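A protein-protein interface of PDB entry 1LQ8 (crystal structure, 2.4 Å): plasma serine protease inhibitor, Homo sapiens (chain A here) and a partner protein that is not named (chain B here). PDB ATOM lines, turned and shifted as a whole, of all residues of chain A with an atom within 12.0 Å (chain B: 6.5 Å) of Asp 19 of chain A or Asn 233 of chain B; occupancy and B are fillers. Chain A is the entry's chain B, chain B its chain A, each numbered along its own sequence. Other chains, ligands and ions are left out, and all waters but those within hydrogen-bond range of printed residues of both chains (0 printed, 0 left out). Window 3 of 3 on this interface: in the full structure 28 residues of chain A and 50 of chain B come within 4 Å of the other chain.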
ATOM      1  N   MET A  15       1.009 -20.867  21.450  1.00  0.00           N
ATOM      2  CA  MET A  15       1.068 -21.170  20.039  1.00  0.00           C
ATOM      3  C   MET A  15       2.354 -20.609  19.476  1.00  0.00           C
ATOM      4  O   MET A  15       2.734 -19.488  19.798  1.00  0.00           O
ATOM      5  CB  MET A  15      -0.097 -20.563  19.276  1.00  0.00           C
ATOM      6  CG  MET A  15      -0.166 -21.130  17.888  1.00  0.00           C
ATOM      7  SD  MET A  15      -0.951 -20.095  16.688  1.00  0.00           S
ATOM      8  CE  MET A  15      -0.872 -21.158  15.213  1.00  0.00           C
ATOM      9  N   PHE A  16       3.030 -21.409  18.655  1.00  0.00           N
ATOM     10  CA  PHE A  16       4.274 -21.006  17.999  1.00  0.00           C
ATOM     11  C   PHE A  16       4.062 -21.200  16.512  1.00  0.00           C
ATOM     12  O   PHE A  16       3.451 -22.184  16.111  1.00  0.00           O
ATOM     13  CB  PHE A  16       5.431 -21.939  18.328  1.00  0.00           C
ATOM     14  CG  PHE A  16       6.107 -21.681  19.628  1.00  0.00           C
ATOM     15  CD1 PHE A  16       5.429 -21.820  20.829  1.00  0.00           C
ATOM     16  CD2 PHE A  16       7.470 -21.420  19.649  1.00  0.00           C
ATOM     17  CE1 PHE A  16       6.104 -21.712  22.030  1.00  0.00           C
ATOM     18  CE2 PHE A  16       8.151 -21.311  20.845  1.00  0.00           C
ATOM     19  CZ  PHE A  16       7.464 -21.461  22.041  1.00  0.00           C
ATOM     20  N   ILE A  17       4.549 -20.289  15.688  1.00  0.00           N
ATOM     21  CA  ILE A  17       4.454 -20.506  14.248  1.00  0.00           C
ATOM     22  C   ILE A  17       5.920 -20.481  13.853  1.00  0.00           C
ATOM     23  O   ILE A  17       6.503 -19.425  13.648  1.00  0.00           O
ATOM     24  CB  ILE A  17       3.662 -19.399  13.516  1.00  0.00           C
ATOM     25  CG1 ILE A  17       2.185 -19.481  13.905  1.00  0.00           C
ATOM     26  CG2 ILE A  17       3.775 -19.592  12.023  1.00  0.00           C
ATOM     27  CD1 ILE A  17       1.298 -18.532  13.156  1.00  0.00           C
ATOM     28  N   VAL A  18       6.530 -21.651  13.777  1.00  0.00           N
ATOM     29  CA  VAL A  18       7.941 -21.694  13.470  1.00  0.00           C
ATOM     30  C   VAL A  18       8.346 -21.968  12.042  1.00  0.00           C
ATOM     31  O   VAL A  18       7.747 -22.774  11.332  1.00  0.00           O
ATOM     32  CB  VAL A  18       8.669 -22.692  14.369  1.00  0.00           C
ATOM     33  CG1 VAL A  18       8.590 -22.224  15.812  1.00  0.00           C
ATOM     34  CG2 VAL A  18       8.060 -24.061  14.213  1.00  0.00           C
ATOM     35  N   ASP A  19       9.391 -21.244  11.669  1.00  0.00           N
ATOM     36  CA  ASP A  19      10.051 -21.266  10.377  1.00  0.00           C
ATOM     37  C   ASP A  19      11.369 -21.870  10.836  1.00  0.00           C
ATOM     38  O   ASP A  19      11.382 -22.890  11.528  1.00  0.00           O
ATOM     39  CB  ASP A  19      10.259 -19.818   9.950  1.00  0.00           C
ATOM     40  CG  ASP A  19      10.752 -19.686   8.549  1.00  0.00           C
ATOM     41  OD1 ASP A  19      10.086 -20.240   7.646  1.00  0.00           O
ATOM     42  OD2 ASP A  19      11.792 -19.018   8.353  1.00  0.00           O
ATOM     43  N   ASN A  20      12.482 -21.255  10.463  1.00  0.00           N
ATOM     44  CA  ASN A  20      13.752 -21.734  10.970  1.00  0.00           C
ATOM     45  C   ASN A  20      13.910 -20.825  12.181  1.00  0.00           C
ATOM     46  O   ASN A  20      14.733 -21.054  13.068  1.00  0.00           O
ATOM     47  CB  ASN A  20      14.890 -21.500   9.981  1.00  0.00           C
ATOM     48  CG  ASN A  20      15.437 -22.797   9.420  1.00  0.00           C
ATOM     49  OD1 ASN A  20      15.496 -23.809  10.122  1.00  0.00           O
ATOM     50  ND2 ASN A  20      15.857 -22.775   8.155  1.00  0.00           N
ATOM     51  N   ASN A  21      13.073 -19.793  12.200  1.00  0.00           N
ATOM     52  CA  ASN A  21      13.046 -18.811  13.271  1.00  0.00           C
ATOM     53  C   ASN A  21      11.652 -18.823  13.870  1.00  0.00           C
ATOM     54  O   ASN A  21      10.744 -19.480  13.355  1.00  0.00           O
ATOM     55  CB  ASN A  21      13.311 -17.416  12.705  1.00  0.00           C
ATOM     56  CG  ASN A  21      14.542 -17.367  11.820  1.00  0.00           C
ATOM     57  OD1 ASN A  21      15.656 -17.137  12.298  1.00  0.00           O
ATOM     58  ND2 ASN A  21      14.347 -17.590  10.521  1.00  0.00           N
ATOM     59  N   ILE A  22      11.475 -18.089  14.957  1.00  0.00           N
ATOM     60  CA  ILE A  22      10.161 -18.005  15.570  1.00  0.00           C
ATOM     61  C   ILE A  22       9.440 -16.822  14.928  1.00  0.00           C
ATOM     62  O   ILE A  22       9.796 -15.666  15.162  1.00  0.00           O
ATOM     63  CB  ILE A  22      10.273 -17.800  17.089  1.00  0.00           C
ATOM     64  CG1 ILE A  22      10.805 -19.084  17.733  1.00  0.00           C
ATOM     65  CG2 ILE A  22       8.911 -17.387  17.676  1.00  0.00           C
ATOM     66  CD1 ILE A  22      11.134 -18.930  19.193  1.00  0.00           C
ATOM     67  N   LEU A  23       8.438 -17.119  14.106  1.00  0.00           N
ATOM     68  CA  LEU A  23       7.661 -16.095  13.404  1.00  0.00           C
ATOM     69  C   LEU A  23       6.581 -15.463  14.265  1.00  0.00           C
ATOM     70  O   LEU A  23       6.432 -14.246  14.289  1.00  0.00           O
ATOM     71  CB  LEU A  23       7.002 -16.703  12.167  1.00  0.00           C
ATOM     72  CG  LEU A  23       7.790 -16.800  10.865  1.00  0.00           C
ATOM     73  CD1 LEU A  23       9.271 -16.724  11.114  1.00  0.00           C
ATOM     74  CD2 LEU A  23       7.389 -18.079  10.175  1.00  0.00           C
ATOM     75  N   PHE A  24       5.814 -16.297  14.953  1.00  0.00           N
ATOM     76  CA  PHE A  24       4.743 -15.806  15.807  1.00  0.00           C
ATOM     77  C   PHE A  24       4.698 -16.581  17.114  1.00  0.00           C
ATOM     78  O   PHE A  24       5.040 -17.767  17.176  1.00  0.00           O
ATOM     79  CB  PHE A  24       3.396 -15.931  15.091  1.00  0.00           C
ATOM     80  CG  PHE A  24       3.279 -15.070  13.869  1.00  0.00           C
ATOM     81  CD1 PHE A  24       2.745 -13.790  13.952  1.00  0.00           C
ATOM     82  CD2 PHE A  24       3.707 -15.537  12.628  1.00  0.00           C
ATOM     83  CE1 PHE A  24       2.634 -12.985  12.821  1.00  0.00           C
ATOM     84  CE2 PHE A  24       3.603 -14.736  11.487  1.00  0.00           C
ATOM     85  CZ  PHE A  24       3.064 -13.459  11.588  1.00  0.00           C
ATOM     86  N   LEU A  25       4.270 -15.905  18.165  1.00  0.00           N
ATOM     87  CA  LEU A  25       4.173 -16.529  19.466  1.00  0.00           C
ATOM     88  C   LEU A  25       3.043 -15.835  20.195  1.00  0.00           C
ATOM     89  O   LEU A  25       2.895 -14.613  20.100  1.00  0.00           O
ATOM     90  CB  LEU A  25       5.486 -16.351  20.238  1.00  0.00           C
ATOM     91  CG  LEU A  25       5.523 -16.892  21.674  1.00  0.00           C
ATOM     92  CD1 LEU A  25       5.372 -18.384  21.649  1.00  0.00           C
ATOM     93  CD2 LEU A  25       6.823 -16.503  22.349  1.00  0.00           C
ATOM     94  N   LEU B  85      17.690 -14.033   5.849  1.00  0.00           N
ATOM     95  CA  LEU B  85      16.280 -14.315   6.067  1.00  0.00           C
ATOM     96  C   LEU B  85      15.438 -13.578   5.020  1.00  0.00           C
ATOM     97  O   LEU B  85      14.683 -14.202   4.273  1.00  0.00           O
ATOM     98  CB  LEU B  85      15.890 -13.891   7.485  1.00  0.00           C
ATOM     99  CG  LEU B  85      14.453 -14.077   7.976  1.00  0.00           C
ATOM    100  CD1 LEU B  85      13.906 -15.434   7.542  1.00  0.00           C
ATOM    101  CD2 LEU B  85      14.443 -13.937   9.489  1.00  0.00           C
ATOM    102  N   GLU B  88      15.993 -15.178   1.563  1.00  0.00           N
ATOM    103  CA  GLU B  88      15.461 -16.522   1.372  1.00  0.00           C
ATOM    104  C   GLU B  88      13.949 -16.542   1.154  1.00  0.00           C
ATOM    105  O   GLU B  88      13.361 -17.608   0.947  1.00  0.00           O
ATOM    106  CB  GLU B  88      15.815 -17.402   2.569  1.00  0.00           C
ATOM    107  CG  GLU B  88      17.285 -17.737   2.674  1.00  0.00           C
ATOM    108  CD  GLU B  88      17.630 -18.450   3.971  1.00  0.00           C
ATOM    109  OE1 GLU B  88      18.819 -18.805   4.160  1.00  0.00           O
ATOM    110  OE2 GLU B  88      16.709 -18.649   4.804  1.00  0.00           O
ATOM    111  N   ASN B  90      10.484 -16.438  -0.609  1.00  0.00           N
ATOM    112  CA  ASN B  90      10.013 -16.827  -1.930  1.00  0.00           C
ATOM    113  C   ASN B  90       8.678 -16.180  -2.221  1.00  0.00           C
ATOM    114  O   ASN B  90       8.001 -15.693  -1.314  1.00  0.00           O
ATOM    115  CB  ASN B  90       9.870 -18.346  -2.014  1.00  0.00           C
ATOM    116  CG  ASN B  90      11.196 -19.059  -1.868  1.00  0.00           C
ATOM    117  OD1 ASN B  90      12.119 -18.846  -2.661  1.00  0.00           O
ATOM    118  ND2 ASN B  90      11.304 -19.910  -0.851  1.00  0.00           N
ATOM    119  N   ARG B  93       3.965 -18.990  -3.057  1.00  0.00           N
ATOM    120  CA  ARG B  93       3.927 -20.317  -3.645  1.00  0.00           C
ATOM    121  C   ARG B  93       2.458 -20.737  -3.708  1.00  0.00           C
ATOM    122  O   ARG B  93       1.563 -19.889  -3.691  1.00  0.00           O
ATOM    123  CB  ARG B  93       4.719 -21.281  -2.767  1.00  0.00           C
ATOM    124  CG  ARG B  93       5.085 -22.593  -3.420  1.00  0.00           C
ATOM    125  CD  ARG B  93       5.211 -23.643  -2.342  1.00  0.00           C
ATOM    126  NE  ARG B  93       5.905 -23.110  -1.172  1.00  0.00           N
ATOM    127  CZ  ARG B  93       5.874 -23.667   0.033  1.00  0.00           C
ATOM    128  NH1 ARG B  93       6.541 -23.114   1.042  1.00  0.00           N
ATOM    129  NH2 ARG B  93       5.167 -24.772   0.230  1.00  0.00           N
ATOM    130  N   PHE B  96       0.760 -21.287   0.293  1.00  0.00           N
ATOM    131  CA  PHE B  96       1.742 -20.885   1.289  1.00  0.00           C
ATOM    132  C   PHE B  96       2.404 -19.568   0.910  1.00  0.00           C
ATOM    133  O   PHE B  96       2.839 -19.372  -0.223  1.00  0.00           O
ATOM    134  CB  PHE B  96       2.817 -21.965   1.472  1.00  0.00           C
ATOM    135  CG  PHE B  96       3.889 -21.592   2.473  1.00  0.00           C
ATOM    136  CD1 PHE B  96       4.927 -20.730   2.118  1.00  0.00           C
ATOM    137  CD2 PHE B  96       3.831 -22.062   3.788  1.00  0.00           C
ATOM    138  CE1 PHE B  96       5.880 -20.341   3.056  1.00  0.00           C
ATOM    139  CE2 PHE B  96       4.785 -21.673   4.731  1.00  0.00           C
ATOM    140  CZ  PHE B  96       5.806 -20.814   4.364  1.00  0.00           C
ATOM    141  N   LEU B  98       4.882 -16.270   2.760  1.00  0.00           N
ATOM    142  CA  LEU B  98       5.517 -15.578   3.866  1.00  0.00           C
ATOM    143  C   LEU B  98       6.302 -14.437   3.271  1.00  0.00           C
ATOM    144  O   LEU B  98       7.148 -14.655   2.415  1.00  0.00           O
ATOM    145  CB  LEU B  98       6.465 -16.502   4.641  1.00  0.00           C
ATOM    146  CG  LEU B  98       7.326 -15.793   5.697  1.00  0.00           C
ATOM    147  CD1 LEU B  98       6.432 -15.133   6.729  1.00  0.00           C
ATOM    148  CD2 LEU B  98       8.266 -16.784   6.365  1.00  0.00           C
ATOM    149  N   PHE B 176       1.760 -13.888   6.779  1.00  0.00           N
ATOM    150  CA  PHE B 176       1.818 -15.333   6.651  1.00  0.00           C
ATOM    151  C   PHE B 176       0.462 -15.978   6.439  1.00  0.00           C
ATOM    152  O   PHE B 176      -0.461 -15.784   7.235  1.00  0.00           O
ATOM    153  CB  PHE B 176       2.476 -15.921   7.907  1.00  0.00           C
ATOM    154  CG  PHE B 176       2.375 -17.417   8.014  1.00  0.00           C
ATOM    155  CD1 PHE B 176       1.336 -18.011   8.716  1.00  0.00           C
ATOM    156  CD2 PHE B 176       3.345 -18.232   7.448  1.00  0.00           C
ATOM    157  CE1 PHE B 176       1.268 -19.399   8.858  1.00  0.00           C
ATOM    158  CE2 PHE B 176       3.287 -19.620   7.582  1.00  0.00           C
ATOM    159  CZ  PHE B 176       2.248 -20.204   8.290  1.00  0.00           C
ATOM    160  N   TYR B 230       2.568 -27.248   8.000  1.00  0.00           N
ATOM    161  CA  TYR B 230       1.868 -26.517   6.965  1.00  0.00           C
ATOM    162  C   TYR B 230       2.334 -27.006   5.594  1.00  0.00           C
ATOM    163  O   TYR B 230       3.361 -27.681   5.474  1.00  0.00           O
ATOM    164  CB  TYR B 230       2.169 -25.017   7.072  1.00  0.00           C
ATOM    165  CG  TYR B 230       1.508 -24.297   8.228  1.00  0.00           C
ATOM    166  CD1 TYR B 230       0.120 -24.147   8.281  1.00  0.00           C
ATOM    167  CD2 TYR B 230       2.271 -23.754   9.261  1.00  0.00           C
ATOM    168  CE1 TYR B 230      -0.488 -23.473   9.335  1.00  0.00           C
ATOM    169  CE2 TYR B 230       1.679 -23.086  10.315  1.00  0.00           C
ATOM    170  CZ  TYR B 230       0.298 -22.949  10.349  1.00  0.00           C
ATOM    171  OH  TYR B 230      -0.297 -22.310  11.412  1.00  0.00           O
ATOM    172  N   GLN B 231       1.547 -26.679   4.571  1.00  0.00           N
ATOM    173  CA  GLN B 231       1.894 -26.998   3.193  1.00  0.00           C
ATOM    174  C   GLN B 231       3.010 -26.006   2.896  1.00  0.00           C
ATOM    175  O   GLN B 231       2.756 -24.901   2.417  1.00  0.00           O
ATOM    176  CB  GLN B 231       0.719 -26.716   2.262  1.00  0.00           C
ATOM    177  CG  GLN B 231      -0.070 -27.935   1.864  1.00  0.00           C
ATOM    178  CD  GLN B 231      -0.436 -27.920   0.392  1.00  0.00           C
ATOM    179  OE1 GLN B 231      -1.038 -28.868  -0.118  1.00  0.00           O
ATOM    180  NE2 GLN B 231      -0.071 -26.839  -0.304  1.00  0.00           N
ATOM    181  N   GLY B 232       4.240 -26.399   3.197  1.00  0.00           N
ATOM    182  CA  GLY B 232       5.367 -25.509   3.003  1.00  0.00           C
ATOM    183  C   GLY B 232       6.217 -25.569   4.248  1.00  0.00           C
ATOM    184  O   GLY B 232       6.063 -26.493   5.051  1.00  0.00           O
ATOM    185  N   ASN B 233       7.100 -24.602   4.442  1.00  0.00           N
ATOM    186  CA  ASN B 233       7.934 -24.680   5.623  1.00  0.00           C
ATOM    187  C   ASN B 233       7.553 -23.760   6.705  1.00  0.00           C
ATOM    188  O   ASN B 233       7.932 -22.590   6.733  1.00  0.00           O
ATOM    189  CB  ASN B 233       9.371 -24.464   5.273  1.00  0.00           C
ATOM    190  CG  ASN B 233       9.782 -25.348   4.177  1.00  0.00           C
ATOM    191  OD1 ASN B 233       9.892 -26.573   4.337  1.00  0.00           O
ATOM    192  ND2 ASN B 233       9.982 -24.729   3.028  1.00  0.00           N
ATOM    193  N   ALA B 234       6.809 -24.332   7.625  1.00  0.00           N
ATOM    194  CA  ALA B 234       6.327 -23.601   8.755  1.00  0.00           C
ATOM    195  C   ALA B 234       5.491 -24.618   9.479  1.00  0.00           C
ATOM    196  O   ALA B 234       4.648 -25.291   8.873  1.00  0.00           O
ATOM    197  CB  ALA B 234       5.482 -22.431   8.293  1.00  0.00           C
ATOM    198  N   THR B 235       5.776 -24.779  10.762  1.00  0.00           N
ATOM    199  CA  THR B 235       5.009 -25.697  11.569  1.00  0.00           C
ATOM    200  C   THR B 235       4.438 -24.922  12.716  1.00  0.00           C
ATOM    201  O   THR B 235       5.079 -24.020  13.245  1.00  0.00           O
ATOM    202  CB  THR B 235       5.841 -26.813  12.205  1.00  0.00           C
ATOM    203  OG1 THR B 235       6.473 -27.598  11.191  1.00  0.00           O
ATOM    204  CG2 THR B 235       4.932 -27.713  13.030  1.00  0.00           C
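The backbone NH of Val 18 of chain A lies within hydrogen-bond range of the backbone carbonyl oxygen of Thr 235 of chain B, 2.8 Å away. The backbone carbonyl oxygen (O) of Asn 233 of chain B sits close to the side-chain carboxylate (OD1) of Asp 19 of chain A (3.3 Å).
N of Ile 17 of chain A is in hydrogen-bond range of O of Phe 24 of chain A, at 3.0 Å. N of Leu 23 of chain A sits at hydrogen-bond distance from O of Ile 17 of chain A (3.0 Å).
Among the printed residues, merely in contact across the chains: Val 18 of chain A with Ala 234 of chain B, Ile 17 of chain A with Thr 235 of chain B, Asn 21 of chain A with Leu 85 of chain B, Phe 16 of chain A with Thr 235 of chain B and Phe 24 of chain A with Phe 176 of chain B.
Printed residues of chain B within 4 Å of Phe 16 of chain A: Thr 235 (3.8 Å). Of the printed residues of chain B, Val 18 of chain A touches Ala 234 and Thr 235. Of the printed residues of chain A, Leu 85 of chain B touches Asn 21 (3.7 Å). Printed residues of chain A within 4 Å of Phe 176 of chain B: Phe 24 (3.9 Å). Tyr 230 of chain B touches none of the printed residues of chain A. No residue of chain A comes within 4 Å of Gly 232 of chain B. Asn 233 of chain B touches just one residue of chain A: Asp 19. Of chain A, only Val 18 (3.1 Å) comes within 4 Å of Ala 234 of chain B. Thr 235 of chain B touches just these residues of chain A: Phe 16, Ile 17 and Val 18. The nearest residue of chain B that does not touch Asp 19 of chain A is Leu 98 of chain B (4.1 Å). The nearest residue of chain A that does not touch Asn 233 of chain B is Val 18 of chain A (4.6 Å).
Of the 11 printed residues of chain A, 6 touch a printed residue of chain B. Hydrophobic or aromatic side chains of chain A within 4 Å of the printed part of chain B: Val 18 and Phe 24. Along chain A the printed residues that touch a printed residue of chain B span positions 16 to 24. Of the 13 printed residues of chain B, 5 touch a printed residue of chain A. Hydrophobic or aromatic side chains of chain B that line the printed part of chain A: Leu 85, Phe 176 and Ala 234. Among the printed residues, 7 pairs touch across the chains. Among the printed residues, no Asp or Glu carboxylate lies within 4 Å of a Lys or Arg side-chain nitrogen of the other chain.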
